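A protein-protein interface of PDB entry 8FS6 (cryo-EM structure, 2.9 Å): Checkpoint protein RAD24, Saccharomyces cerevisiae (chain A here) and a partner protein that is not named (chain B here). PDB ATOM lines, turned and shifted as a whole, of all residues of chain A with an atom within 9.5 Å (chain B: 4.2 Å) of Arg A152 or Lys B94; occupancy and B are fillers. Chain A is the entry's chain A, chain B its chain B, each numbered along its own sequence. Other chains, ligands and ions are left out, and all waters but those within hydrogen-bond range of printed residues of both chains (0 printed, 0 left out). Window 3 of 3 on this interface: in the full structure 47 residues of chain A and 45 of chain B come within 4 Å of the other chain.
Among the printed residues, pairs that only touch across the chains: Asp A188 with Arg B129 (3.2 Å), Ile A156 with Asn B91 (3.3 Å), Arg A152 with Arg B129 (3.4 Å) and Arg A152 with Lys B94 (3.6 Å).
Along chain A the printed residues that touch a printed residue of chain B span positions 151 to 188.
Among the printed residues, 7 pairs touch across the chains.
Among the printed residues, no Asp or Glu carboxylate lies within 4 Å of a Lys or Arg side-chain nitrogen of the other chain.
The backbone carbonyl oxygen (O) of Asp A154 sits at hydrogen-bond distance from the guanidinium group (NH2) of Arg A152.
ND1 of His B95 lies close to O of Asn B91, 3.4 Å away.
The backbone NH (N) of Phe A151 sits at hydrogen-bond distance from the backbone carbonyl oxygen (O) of Leu A185 (3.3 Å).
The backbone carbonyl oxygen (O) of Val B89 sits at hydrogen-bond distance from the backbone NH (N) of Lys B94 (3.5 Å).
Arg A152 touches just these residues of chain B: Lys B94 (3.6 Å) and Arg B129 (3.4 Å).
Of chain A, only Arg A152 (3.6 Å) and Asp A154 (3.0 Å) come within 4 Å of Lys B94.
Of the printed residues of chain B, Asp A188 touches Arg B129 (3.2 Å).
Of the printed residues of chain B, Ile A156 touches Asn B91 (3.3 Å).
Printed residues of chain A within 4 Å of Asn B91: Ile A156.
Of the printed residues of chain A, Arg B129 touches Phe A151 (3.4 Å), Arg A152 (3.4 Å) and Asp A188 (3.2 Å).
Of the printed residues of chain B, Asp A154 touches Lys B94.
Ser A165 touches none of the printed residues of chain B.
The nearest residue of chain A that does not touch Lys B94 is Cys A155 (5.1 Å).
The guanidinium group of Arg B129 sits at hydrogen-bond distance from the backbone carbonyl oxygen of Phe A151 (3.4 Å).
OE1 of Gln A162 lies close to NH1 of Arg B90, at 2.3 Å.
The backbone carbonyl oxygen (O) of Asp A154 sits at hydrogen-bond distance from the side-chain amino group (NZ) of Lys B94 (3.0 Å).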
ATOM      1  N   THR A 149     -28.017   7.469   1.243  1.00  0.00           N
ATOM      2  CA  THR A 149     -28.668   6.658   2.269  1.00  0.00           C
ATOM      3  C   THR A 149     -27.891   6.851   3.569  1.00  0.00           C
ATOM      4  O   THR A 149     -26.910   6.152   3.834  1.00  0.00           O
ATOM      5  CB  THR A 149     -28.722   5.187   1.862  1.00  0.00           C
ATOM      6  OG1 THR A 149     -29.311   5.071   0.561  1.00  0.00           O
ATOM      7  CG2 THR A 149     -29.544   4.384   2.862  1.00  0.00           C
ATOM      8  N   GLU A 150     -28.333   7.810   4.378  1.00  0.00           N
ATOM      9  CA  GLU A 150     -27.650   8.124   5.624  1.00  0.00           C
ATOM     10  C   GLU A 150     -27.960   7.078   6.689  1.00  0.00           C
ATOM     11  O   GLU A 150     -29.094   6.606   6.807  1.00  0.00           O
ATOM     12  CB  GLU A 150     -28.066   9.502   6.141  1.00  0.00           C
ATOM     13  CG  GLU A 150     -27.568  10.715   5.363  1.00  0.00           C
ATOM     14  CD  GLU A 150     -28.656  11.321   4.503  1.00  0.00           C
ATOM     15  OE1 GLU A 150     -29.841  11.151   4.845  1.00  0.00           O
ATOM     16  OE2 GLU A 150     -28.337  12.036   3.534  1.00  0.00           O
ATOM     17  N   PHE A 151     -26.944   6.728   7.475  1.00  0.00           N
ATOM     18  CA  PHE A 151     -27.150   5.843   8.614  1.00  0.00           C
ATOM     19  C   PHE A 151     -27.686   6.638   9.798  1.00  0.00           C
ATOM     20  O   PHE A 151     -27.151   7.697  10.142  1.00  0.00           O
ATOM     21  CB  PHE A 151     -25.844   5.145   8.989  1.00  0.00           C
ATOM     22  CG  PHE A 151     -25.863   4.521  10.356  1.00  0.00           C
ATOM     23  CD1 PHE A 151     -26.672   3.428  10.623  1.00  0.00           C
ATOM     24  CD2 PHE A 151     -25.071   5.026  11.374  1.00  0.00           C
ATOM     25  CE1 PHE A 151     -26.691   2.853  11.879  1.00  0.00           C
ATOM     26  CE2 PHE A 151     -25.085   4.455  12.631  1.00  0.00           C
ATOM     27  CZ  PHE A 151     -25.896   3.366  12.885  1.00  0.00           C
ATOM     28  N   ARG A 152     -28.744   6.129  10.422  1.00  0.00           N
ATOM     29  CA  ARG A 152     -29.383   6.784  11.555  1.00  0.00           C
ATOM     30  C   ARG A 152     -29.036   6.022  12.827  1.00  0.00           C
ATOM     31  O   ARG A 152     -29.431   4.863  12.988  1.00  0.00           O
ATOM     32  CB  ARG A 152     -30.898   6.854  11.359  1.00  0.00           C
ATOM     33  CG  ARG A 152     -31.359   8.074  10.575  1.00  0.00           C
ATOM     34  CD  ARG A 152     -32.870   8.274  10.642  1.00  0.00           C
ATOM     35  NE  ARG A 152     -33.462   7.750  11.867  1.00  0.00           N
ATOM     36  CZ  ARG A 152     -34.235   6.673  11.926  1.00  0.00           C
ATOM     37  NH1 ARG A 152     -34.530   5.974  10.842  1.00  0.00           N
ATOM     38  NH2 ARG A 152     -34.723   6.289  13.101  1.00  0.00           N
ATOM     39  N   GLY A 153     -28.292   6.675  13.722  1.00  0.00           N
ATOM     40  CA  GLY A 153     -27.892   6.019  14.957  1.00  0.00           C
ATOM     41  C   GLY A 153     -29.056   5.758  15.894  1.00  0.00           C
ATOM     42  O   GLY A 153     -29.124   4.704  16.533  1.00  0.00           O
ATOM     43  N   ASP A 154     -29.985   6.709  15.992  1.00  0.00           N
ATOM     44  CA  ASP A 154     -31.123   6.591  16.904  1.00  0.00           C
ATOM     45  C   ASP A 154     -32.247   5.803  16.230  1.00  0.00           C
ATOM     46  O   ASP A 154     -33.295   6.331  15.851  1.00  0.00           O
ATOM     47  CB  ASP A 154     -31.589   7.970  17.354  1.00  0.00           C
ATOM     48  CG  ASP A 154     -31.574   8.987  16.229  1.00  0.00           C
ATOM     49  OD1 ASP A 154     -30.905   8.736  15.205  1.00  0.00           O
ATOM     50  OD2 ASP A 154     -32.229  10.042  16.371  1.00  0.00           O
ATOM     51  N   CYS A 155     -32.003   4.500  16.085  1.00  0.00           N
ATOM     52  CA  CYS A 155     -32.973   3.566  15.503  1.00  0.00           C
ATOM     53  C   CYS A 155     -32.916   2.287  16.337  1.00  0.00           C
ATOM     54  O   CYS A 155     -32.089   1.406  16.087  1.00  0.00           O
ATOM     55  CB  CYS A 155     -32.677   3.300  14.033  1.00  0.00           C
ATOM     56  SG  CYS A 155     -33.824   2.151  13.236  1.00  0.00           S
ATOM     57  N   ILE A 156     -33.803   2.192  17.326  1.00  0.00           N
ATOM     58  CA  ILE A 156     -33.809   1.066  18.262  1.00  0.00           C
ATOM     59  C   ILE A 156     -34.810   0.047  17.727  1.00  0.00           C
ATOM     60  O   ILE A 156     -36.009   0.109  18.002  1.00  0.00           O
ATOM     61  CB  ILE A 156     -34.130   1.509  19.687  1.00  0.00           C
ATOM     62  CG1 ILE A 156     -33.237   2.685  20.090  1.00  0.00           C
ATOM     63  CG2 ILE A 156     -33.957   0.347  20.656  1.00  0.00           C
ATOM     64  CD1 ILE A 156     -33.384   3.098  21.538  1.00  0.00           C
ATOM     65  N   VAL A 157     -34.303  -0.906  16.944  1.00  0.00           N
ATOM     66  CA  VAL A 157     -35.128  -2.008  16.464  1.00  0.00           C
ATOM     67  C   VAL A 157     -35.360  -2.993  17.608  1.00  0.00           C
ATOM     68  O   VAL A 157     -34.487  -3.205  18.461  1.00  0.00           O
ATOM     69  CB  VAL A 157     -34.451  -2.669  15.245  1.00  0.00           C
ATOM     70  CG1 VAL A 157     -34.903  -4.107  15.049  1.00  0.00           C
ATOM     71  CG2 VAL A 157     -34.717  -1.850  13.988  1.00  0.00           C
ATOM     72  N   LEU A 160     -32.991  -6.328  18.276  1.00  0.00           N
ATOM     73  CA  LEU A 160     -31.690  -5.921  17.683  1.00  0.00           C
ATOM     74  C   LEU A 160     -30.817  -5.283  18.763  1.00  0.00           C
ATOM     75  O   LEU A 160     -31.025  -4.092  19.058  1.00  0.00           O
ATOM     76  CB  LEU A 160     -31.919  -4.936  16.533  1.00  0.00           C
ATOM     77  CG  LEU A 160     -30.661  -4.526  15.770  1.00  0.00           C
ATOM     78  CD1 LEU A 160     -30.011  -5.730  15.108  1.00  0.00           C
ATOM     79  CD2 LEU A 160     -30.979  -3.460  14.738  1.00  0.00           C
ATOM     80  N   GLN A 162     -27.892  -3.217  20.550  1.00  0.00           N
ATOM     81  CA  GLN A 162     -27.401  -1.919  20.101  1.00  0.00           C
ATOM     82  C   GLN A 162     -25.991  -1.966  19.517  1.00  0.00           C
ATOM     83  O   GLN A 162     -25.433  -0.907  19.212  1.00  0.00           O
ATOM     84  CB  GLN A 162     -27.452  -0.911  21.251  1.00  0.00           C
ATOM     85  CG  GLN A 162     -28.614   0.073  21.168  1.00  0.00           C
ATOM     86  CD  GLN A 162     -28.571   0.935  19.917  1.00  0.00           C
ATOM     87  OE1 GLN A 162     -27.974   2.010  19.914  1.00  0.00           O
ATOM     88  NE2 GLN A 162     -29.224   0.476  18.854  1.00  0.00           N
ATOM     89  N   SER A 165     -26.745  -2.796  15.069  1.00  0.00           N
ATOM     90  CA  SER A 165     -27.482  -1.878  14.205  1.00  0.00           C
ATOM     91  C   SER A 165     -26.661  -1.503  12.976  1.00  0.00           C
ATOM     92  O   SER A 165     -27.163  -1.538  11.846  1.00  0.00           O
ATOM     93  CB  SER A 165     -27.884  -0.629  14.989  1.00  0.00           C
ATOM     94  OG  SER A 165     -26.743   0.090  15.424  1.00  0.00           O
ATOM     95  N   PHE A 166     -25.386  -1.159  13.177  1.00  0.00           N
ATOM     96  CA  PHE A 166     -24.528  -0.840  12.042  1.00  0.00           C
ATOM     97  C   PHE A 166     -24.260  -2.064  11.177  1.00  0.00           C
ATOM     98  O   PHE A 166     -24.134  -1.938   9.954  1.00  0.00           O
ATOM     99  CB  PHE A 166     -23.207  -0.237  12.515  1.00  0.00           C
ATOM    100  CG  PHE A 166     -22.354   0.284  11.397  1.00  0.00           C
ATOM    101  CD1 PHE A 166     -22.796   1.329  10.602  1.00  0.00           C
ATOM    102  CD2 PHE A 166     -21.124  -0.287  11.121  1.00  0.00           C
ATOM    103  CE1 PHE A 166     -22.018   1.807   9.566  1.00  0.00           C
ATOM    104  CE2 PHE A 166     -20.343   0.184  10.085  1.00  0.00           C
ATOM    105  CZ  PHE A 166     -20.790   1.233   9.305  1.00  0.00           C
ATOM    106  N   PHE A 169     -27.255  -2.426   9.070  1.00  0.00           N
ATOM    107  CA  PHE A 169     -27.246  -1.356   8.078  1.00  0.00           C
ATOM    108  C   PHE A 169     -26.292  -1.673   6.932  1.00  0.00           C
ATOM    109  O   PHE A 169     -26.624  -1.458   5.760  1.00  0.00           O
ATOM    110  CB  PHE A 169     -26.867  -0.032   8.742  1.00  0.00           C
ATOM    111  CG  PHE A 169     -26.712   1.109   7.778  1.00  0.00           C
ATOM    112  CD1 PHE A 169     -27.824   1.748   7.258  1.00  0.00           C
ATOM    113  CD2 PHE A 169     -25.454   1.547   7.397  1.00  0.00           C
ATOM    114  CE1 PHE A 169     -27.687   2.798   6.371  1.00  0.00           C
ATOM    115  CE2 PHE A 169     -25.310   2.596   6.512  1.00  0.00           C
ATOM    116  CZ  PHE A 169     -26.428   3.223   5.998  1.00  0.00           C
ATOM    117  N   ILE A 184     -23.875   5.442  -0.027  1.00  0.00           N
ATOM    118  CA  ILE A 184     -24.139   5.383   1.408  1.00  0.00           C
ATOM    119  C   ILE A 184     -23.237   6.381   2.122  1.00  0.00           C
ATOM    120  O   ILE A 184     -22.010   6.340   1.979  1.00  0.00           O
ATOM    121  CB  ILE A 184     -23.934   3.962   1.951  1.00  0.00           C
ATOM    122  CG1 ILE A 184     -24.981   3.017   1.363  1.00  0.00           C
ATOM    123  CG2 ILE A 184     -24.010   3.958   3.467  1.00  0.00           C
ATOM    124  CD1 ILE A 184     -24.424   2.052   0.359  1.00  0.00           C
ATOM    125  N   LEU A 185     -23.845   7.278   2.891  1.00  0.00           N
ATOM    126  CA  LEU A 185     -23.131   8.287   3.658  1.00  0.00           C
ATOM    127  C   LEU A 185     -23.262   7.973   5.142  1.00  0.00           C
ATOM    128  O   LEU A 185     -24.370   7.744   5.636  1.00  0.00           O
ATOM    129  CB  LEU A 185     -23.677   9.685   3.361  1.00  0.00           C
ATOM    130  CG  LEU A 185     -23.148  10.836   4.220  1.00  0.00           C
ATOM    131  CD1 LEU A 185     -21.638  10.937   4.114  1.00  0.00           C
ATOM    132  CD2 LEU A 185     -23.805  12.148   3.824  1.00  0.00           C
ATOM    133  N   ILE A 186     -22.136   7.960   5.844  1.00  0.00           N
ATOM    134  CA  ILE A 186     -22.110   7.718   7.285  1.00  0.00           C
ATOM    135  C   ILE A 186     -21.565   8.987   7.930  1.00  0.00           C
ATOM    136  O   ILE A 186     -20.353   9.159   8.093  1.00  0.00           O
ATOM    137  CB  ILE A 186     -21.274   6.493   7.661  1.00  0.00           C
ATOM    138  CG1 ILE A 186     -21.692   5.281   6.828  1.00  0.00           C
ATOM    139  CG2 ILE A 186     -21.411   6.188   9.145  1.00  0.00           C
ATOM    140  CD1 ILE A 186     -20.799   4.077   7.018  1.00  0.00           C
ATOM    141  N   GLU A 187     -22.468   9.892   8.309  1.00  0.00           N
ATOM    142  CA  GLU A 187     -22.080  11.096   9.031  1.00  0.00           C
ATOM    143  C   GLU A 187     -22.174  10.909  10.539  1.00  0.00           C
ATOM    144  O   GLU A 187     -21.197  11.156  11.256  1.00  0.00           O
ATOM    145  CB  GLU A 187     -22.949  12.280   8.602  1.00  0.00           C
ATOM    146  CG  GLU A 187     -22.237  13.621   8.671  1.00  0.00           C
ATOM    147  CD  GLU A 187     -23.193  14.795   8.584  1.00  0.00           C
ATOM    148  OE1 GLU A 187     -24.420  14.565   8.580  1.00  0.00           O
ATOM    149  OE2 GLU A 187     -22.716  15.948   8.526  1.00  0.00           O
ATOM    150  N   ASP A 188     -23.330  10.475  11.035  1.00  0.00           N
ATOM    151  CA  ASP A 188     -23.500  10.170  12.454  1.00  0.00           C
ATOM    152  C   ASP A 188     -22.983   8.758  12.689  1.00  0.00           C
ATOM    153  O   ASP A 188     -23.689   7.775  12.452  1.00  0.00           O
ATOM    154  CB  ASP A 188     -24.956  10.312  12.877  1.00  0.00           C
ATOM    155  CG  ASP A 188     -25.101  10.905  14.263  1.00  0.00           C
ATOM    156  OD1 ASP A 188     -24.240  11.719  14.656  1.00  0.00           O
ATOM    157  OD2 ASP A 188     -26.082  10.562  14.958  1.00  0.00           O
ATOM    158  N   LEU A 189     -21.743   8.662  13.154  1.00  0.00           N
ATOM    159  CA  LEU A 189     -21.131   7.379  13.426  1.00  0.00           C
ATOM    160  C   LEU A 189     -21.799   6.725  14.632  1.00  0.00           C
ATOM    161  O   LEU A 189     -22.425   7.403  15.450  1.00  0.00           O
ATOM    162  CB  LEU A 189     -19.636   7.561  13.675  1.00  0.00           C
ATOM    163  CG  LEU A 189     -18.973   8.594  12.761  1.00  0.00           C
ATOM    164  CD1 LEU A 189     -17.753   9.204  13.424  1.00  0.00           C
ATOM    165  CD2 LEU A 189     -18.605   7.975  11.424  1.00  0.00           C
ATOM    166  N   PRO A 190     -21.693   5.393  14.758  1.00  0.00           N
ATOM    167  CA  PRO A 190     -22.213   4.728  15.961  1.00  0.00           C
ATOM    168  C   PRO A 190     -21.499   5.181  17.227  1.00  0.00           C
ATOM    169  O   PRO A 190     -20.540   5.957  17.162  1.00  0.00           O
ATOM    170  CB  PRO A 190     -21.962   3.242  15.675  1.00  0.00           C
ATOM    171  CG  PRO A 190     -21.943   3.150  14.187  1.00  0.00           C
ATOM    172  CD  PRO A 190     -21.295   4.423  13.725  1.00  0.00           C
ATOM    173  N   ASN A 191     -21.942   4.693  18.384  1.00  0.00           N
ATOM    174  CA  ASN A 191     -21.410   5.153  19.666  1.00  0.00           C
ATOM    175  C   ASN A 191     -19.994   4.607  19.823  1.00  0.00           C
ATOM    176  O   ASN A 191     -19.740   3.613  20.507  1.00  0.00           O
ATOM    177  CB  ASN A 191     -22.312   4.717  20.814  1.00  0.00           C
ATOM    178  CG  ASN A 191     -21.932   5.365  22.130  1.00  0.00           C
ATOM    179  OD1 ASN A 191     -21.208   6.360  22.160  1.00  0.00           O
ATOM    180  ND2 ASN A 191     -22.421   4.803  23.229  1.00  0.00           N
ATOM    181  N   VAL B  89     -30.967  10.510  25.672  1.00  0.00           N
ATOM    182  CA  VAL B  89     -30.956  11.339  24.469  1.00  0.00           C
ATOM    183  C   VAL B  89     -31.643  10.617  23.315  1.00  0.00           C
ATOM    184  O   VAL B  89     -32.413  11.219  22.555  1.00  0.00           O
ATOM    185  CB  VAL B  89     -29.513  11.740  24.109  1.00  0.00           C
ATOM    186  CG1 VAL B  89     -29.473  12.447  22.765  1.00  0.00           C
ATOM    187  CG2 VAL B  89     -28.928  12.633  25.191  1.00  0.00           C
ATOM    188  N   ARG B  90     -31.391   9.314  23.175  1.00  0.00           N
ATOM    189  CA  ARG B  90     -31.962   8.558  22.069  1.00  0.00           C
ATOM    190  C   ARG B  90     -33.444   8.250  22.245  1.00  0.00           C
ATOM    191  O   ARG B  90     -34.119   7.966  21.250  1.00  0.00           O
ATOM    192  CB  ARG B  90     -31.189   7.251  21.872  1.00  0.00           C
ATOM    193  CG  ARG B  90     -29.861   7.428  21.153  1.00  0.00           C
ATOM    194  CD  ARG B  90     -29.199   6.092  20.864  1.00  0.00           C
ATOM    195  NE  ARG B  90     -29.079   5.269  22.062  1.00  0.00           N
ATOM    196  CZ  ARG B  90     -28.261   4.232  22.178  1.00  0.00           C
ATOM    197  NH1 ARG B  90     -27.464   3.868  21.188  1.00  0.00           N
ATOM    198  NH2 ARG B  90     -28.240   3.546  23.317  1.00  0.00           N
ATOM    199  N   ASN B  91     -33.971   8.288  23.471  1.00  0.00           N
ATOM    200  CA  ASN B  91     -35.372   7.946  23.690  1.00  0.00           C
ATOM    201  C   ASN B  91     -36.222   9.136  24.121  1.00  0.00           C
ATOM    202  O   ASN B  91     -37.139   9.527  23.396  1.00  0.00           O
ATOM    203  CB  ASN B  91     -35.471   6.826  24.736  1.00  0.00           C
ATOM    204  CG  ASN B  91     -35.251   5.452  24.139  1.00  0.00           C
ATOM    205  OD1 ASN B  91     -35.428   5.248  22.939  1.00  0.00           O
ATOM    206  ND2 ASN B  91     -34.861   4.498  24.977  1.00  0.00           N
ATOM    207  N   GLN B  92     -35.916   9.758  25.261  1.00  0.00           N
ATOM    208  CA  GLN B  92     -36.802  10.780  25.811  1.00  0.00           C
ATOM    209  C   GLN B  92     -36.725  12.076  25.012  1.00  0.00           C
ATOM    210  O   GLN B  92     -37.758  12.663  24.669  1.00  0.00           O
ATOM    211  CB  GLN B  92     -36.456  11.033  27.280  1.00  0.00           C
ATOM    212  CG  GLN B  92     -37.390  12.004  27.983  1.00  0.00           C
ATOM    213  CD  GLN B  92     -36.986  12.258  29.421  1.00  0.00           C
ATOM    214  OE1 GLN B  92     -36.004  11.699  29.910  1.00  0.00           O
ATOM    215  NE2 GLN B  92     -37.745  13.104  30.109  1.00  0.00           N
ATOM    216  N   ILE B  93     -35.508  12.531  24.704  1.00  0.00           N
ATOM    217  CA  ILE B  93     -35.346  13.745  23.911  1.00  0.00           C
ATOM    218  C   ILE B  93     -35.893  13.535  22.506  1.00  0.00           C
ATOM    219  O   ILE B  93     -36.530  14.426  21.931  1.00  0.00           O
ATOM    220  CB  ILE B  93     -33.868  14.178  23.888  1.00  0.00           C
ATOM    221  CG1 ILE B  93     -33.331  14.307  25.314  1.00  0.00           C
ATOM    222  CG2 ILE B  93     -33.707  15.492  23.137  1.00  0.00           C
ATOM    223  CD1 ILE B  93     -31.933  14.883  25.394  1.00  0.00           C
ATOM    224  N   LYS B  94     -35.663  12.348  21.936  1.00  0.00           N
ATOM    225  CA  LYS B  94     -36.184  12.048  20.607  1.00  0.00           C
ATOM    226  C   LYS B  94     -37.708  12.057  20.591  1.00  0.00           C
ATOM    227  O   LYS B  94     -38.321  12.607  19.669  1.00  0.00           O
ATOM    228  CB  LYS B  94     -35.649  10.699  20.128  1.00  0.00           C
ATOM    229  CG  LYS B  94     -36.345  10.162  18.887  1.00  0.00           C
ATOM    230  CD  LYS B  94     -35.733   8.850  18.430  1.00  0.00           C
ATOM    231  CE  LYS B  94     -35.278   8.932  16.983  1.00  0.00           C
ATOM    232  NZ  LYS B  94     -35.849   7.833  16.157  1.00  0.00           N
ATOM    233  N   HIS B  95     -38.341  11.465  21.608  1.00  0.00           N
ATOM    234  CA  HIS B  95     -39.799  11.435  21.645  1.00  0.00           C
ATOM    235  C   HIS B  95     -40.386  12.812  21.926  1.00  0.00           C
ATOM    236  O   HIS B  95     -41.469  13.132  21.422  1.00  0.00           O
ATOM    237  CB  HIS B  95     -40.277  10.424  22.688  1.00  0.00           C
ATOM    238  CG  HIS B  95     -39.941   9.006  22.348  1.00  0.00           C
ATOM    239  ND1 HIS B  95     -39.522   8.621  21.093  1.00  0.00           N
ATOM    240  CD2 HIS B  95     -39.956   7.880  23.101  1.00  0.00           C
ATOM    241  CE1 HIS B  95     -39.295   7.320  21.086  1.00  0.00           C
ATOM    242  NE2 HIS B  95     -39.551   6.846  22.292  1.00  0.00           N
ATOM    243  N   PHE B  96     -39.701  13.634  22.725  1.00  0.00           N
ATOM    244  CA  PHE B  96     -40.166  15.001  22.932  1.00  0.00           C
ATOM    245  C   PHE B  96     -40.026  15.834  21.664  1.00  0.00           C
ATOM    246  O   PHE B  96     -40.882  16.682  21.385  1.00  0.00           O
ATOM    247  CB  PHE B  96     -39.402  15.652  24.084  1.00  0.00           C
ATOM    248  CG  PHE B  96     -39.809  17.073  24.352  1.00  0.00           C
ATOM    249  CD1 PHE B  96     -41.023  17.356  24.957  1.00  0.00           C
ATOM    250  CD2 PHE B  96     -38.981  18.125  24.001  1.00  0.00           C
ATOM    251  CE1 PHE B  96     -41.404  18.660  25.205  1.00  0.00           C
ATOM    252  CE2 PHE B  96     -39.355  19.432  24.247  1.00  0.00           C
ATOM    253  CZ  PHE B  96     -40.568  19.700  24.850  1.00  0.00           C
ATOM    254  N   ALA B  97     -38.958  15.615  20.894  1.00  0.00           N
ATOM    255  CA  ALA B  97     -38.797  16.322  19.629  1.00  0.00           C
ATOM    256  C   ALA B  97     -39.827  15.865  18.603  1.00  0.00           C
ATOM    257  O   ALA B  97     -40.338  16.677  17.823  1.00  0.00           O
ATOM    258  CB  ALA B  97     -37.380  16.117  19.095  1.00  0.00           C
ATOM    259  N   GLN B  98     -40.147  14.570  18.590  1.00  0.00           N
ATOM    260  CA  GLN B  98     -41.126  14.026  17.659  1.00  0.00           C
ATOM    261  C   GLN B  98     -42.560  14.385  18.025  1.00  0.00           C
ATOM    262  O   GLN B  98     -43.464  14.136  17.221  1.00  0.00           O
ATOM    263  CB  GLN B  98     -40.991  12.504  17.577  1.00  0.00           C
ATOM    264  CG  GLN B  98     -39.756  12.027  16.834  1.00  0.00           C
ATOM    265  CD  GLN B  98     -39.625  10.517  16.833  1.00  0.00           C
ATOM    266  OE1 GLN B  98     -39.997   9.849  17.798  1.00  0.00           O
ATOM    267  NE2 GLN B  98     -39.091   9.970  15.747  1.00  0.00           N
ATOM    268  N   ARG B 129     -27.428  14.747  16.008  1.00  0.00           N
ATOM    269  CA  ARG B 129     -28.476  14.291  15.101  1.00  0.00           C
ATOM    270  C   ARG B 129     -29.849  14.735  15.583  1.00  0.00           C
ATOM    271  O   ARG B 129     -30.747  14.997  14.772  1.00  0.00           O
ATOM    272  CB  ARG B 129     -28.427  12.769  14.965  1.00  0.00           C
ATOM    273  CG  ARG B 129     -29.243  12.213  13.808  1.00  0.00           C
ATOM    274  CD  ARG B 129     -29.045  13.034  12.542  1.00  0.00           C
ATOM    275  NE  ARG B 129     -29.503  12.335  11.346  1.00  0.00           N
ATOM    276  CZ  ARG B 129     -28.885  11.304  10.786  1.00  0.00           C
ATOM    277  NH1 ARG B 129     -27.754  10.824  11.275  1.00  0.00           N
ATOM    278  NH2 ARG B 129     -29.412  10.744   9.701  1.00  0.00           N
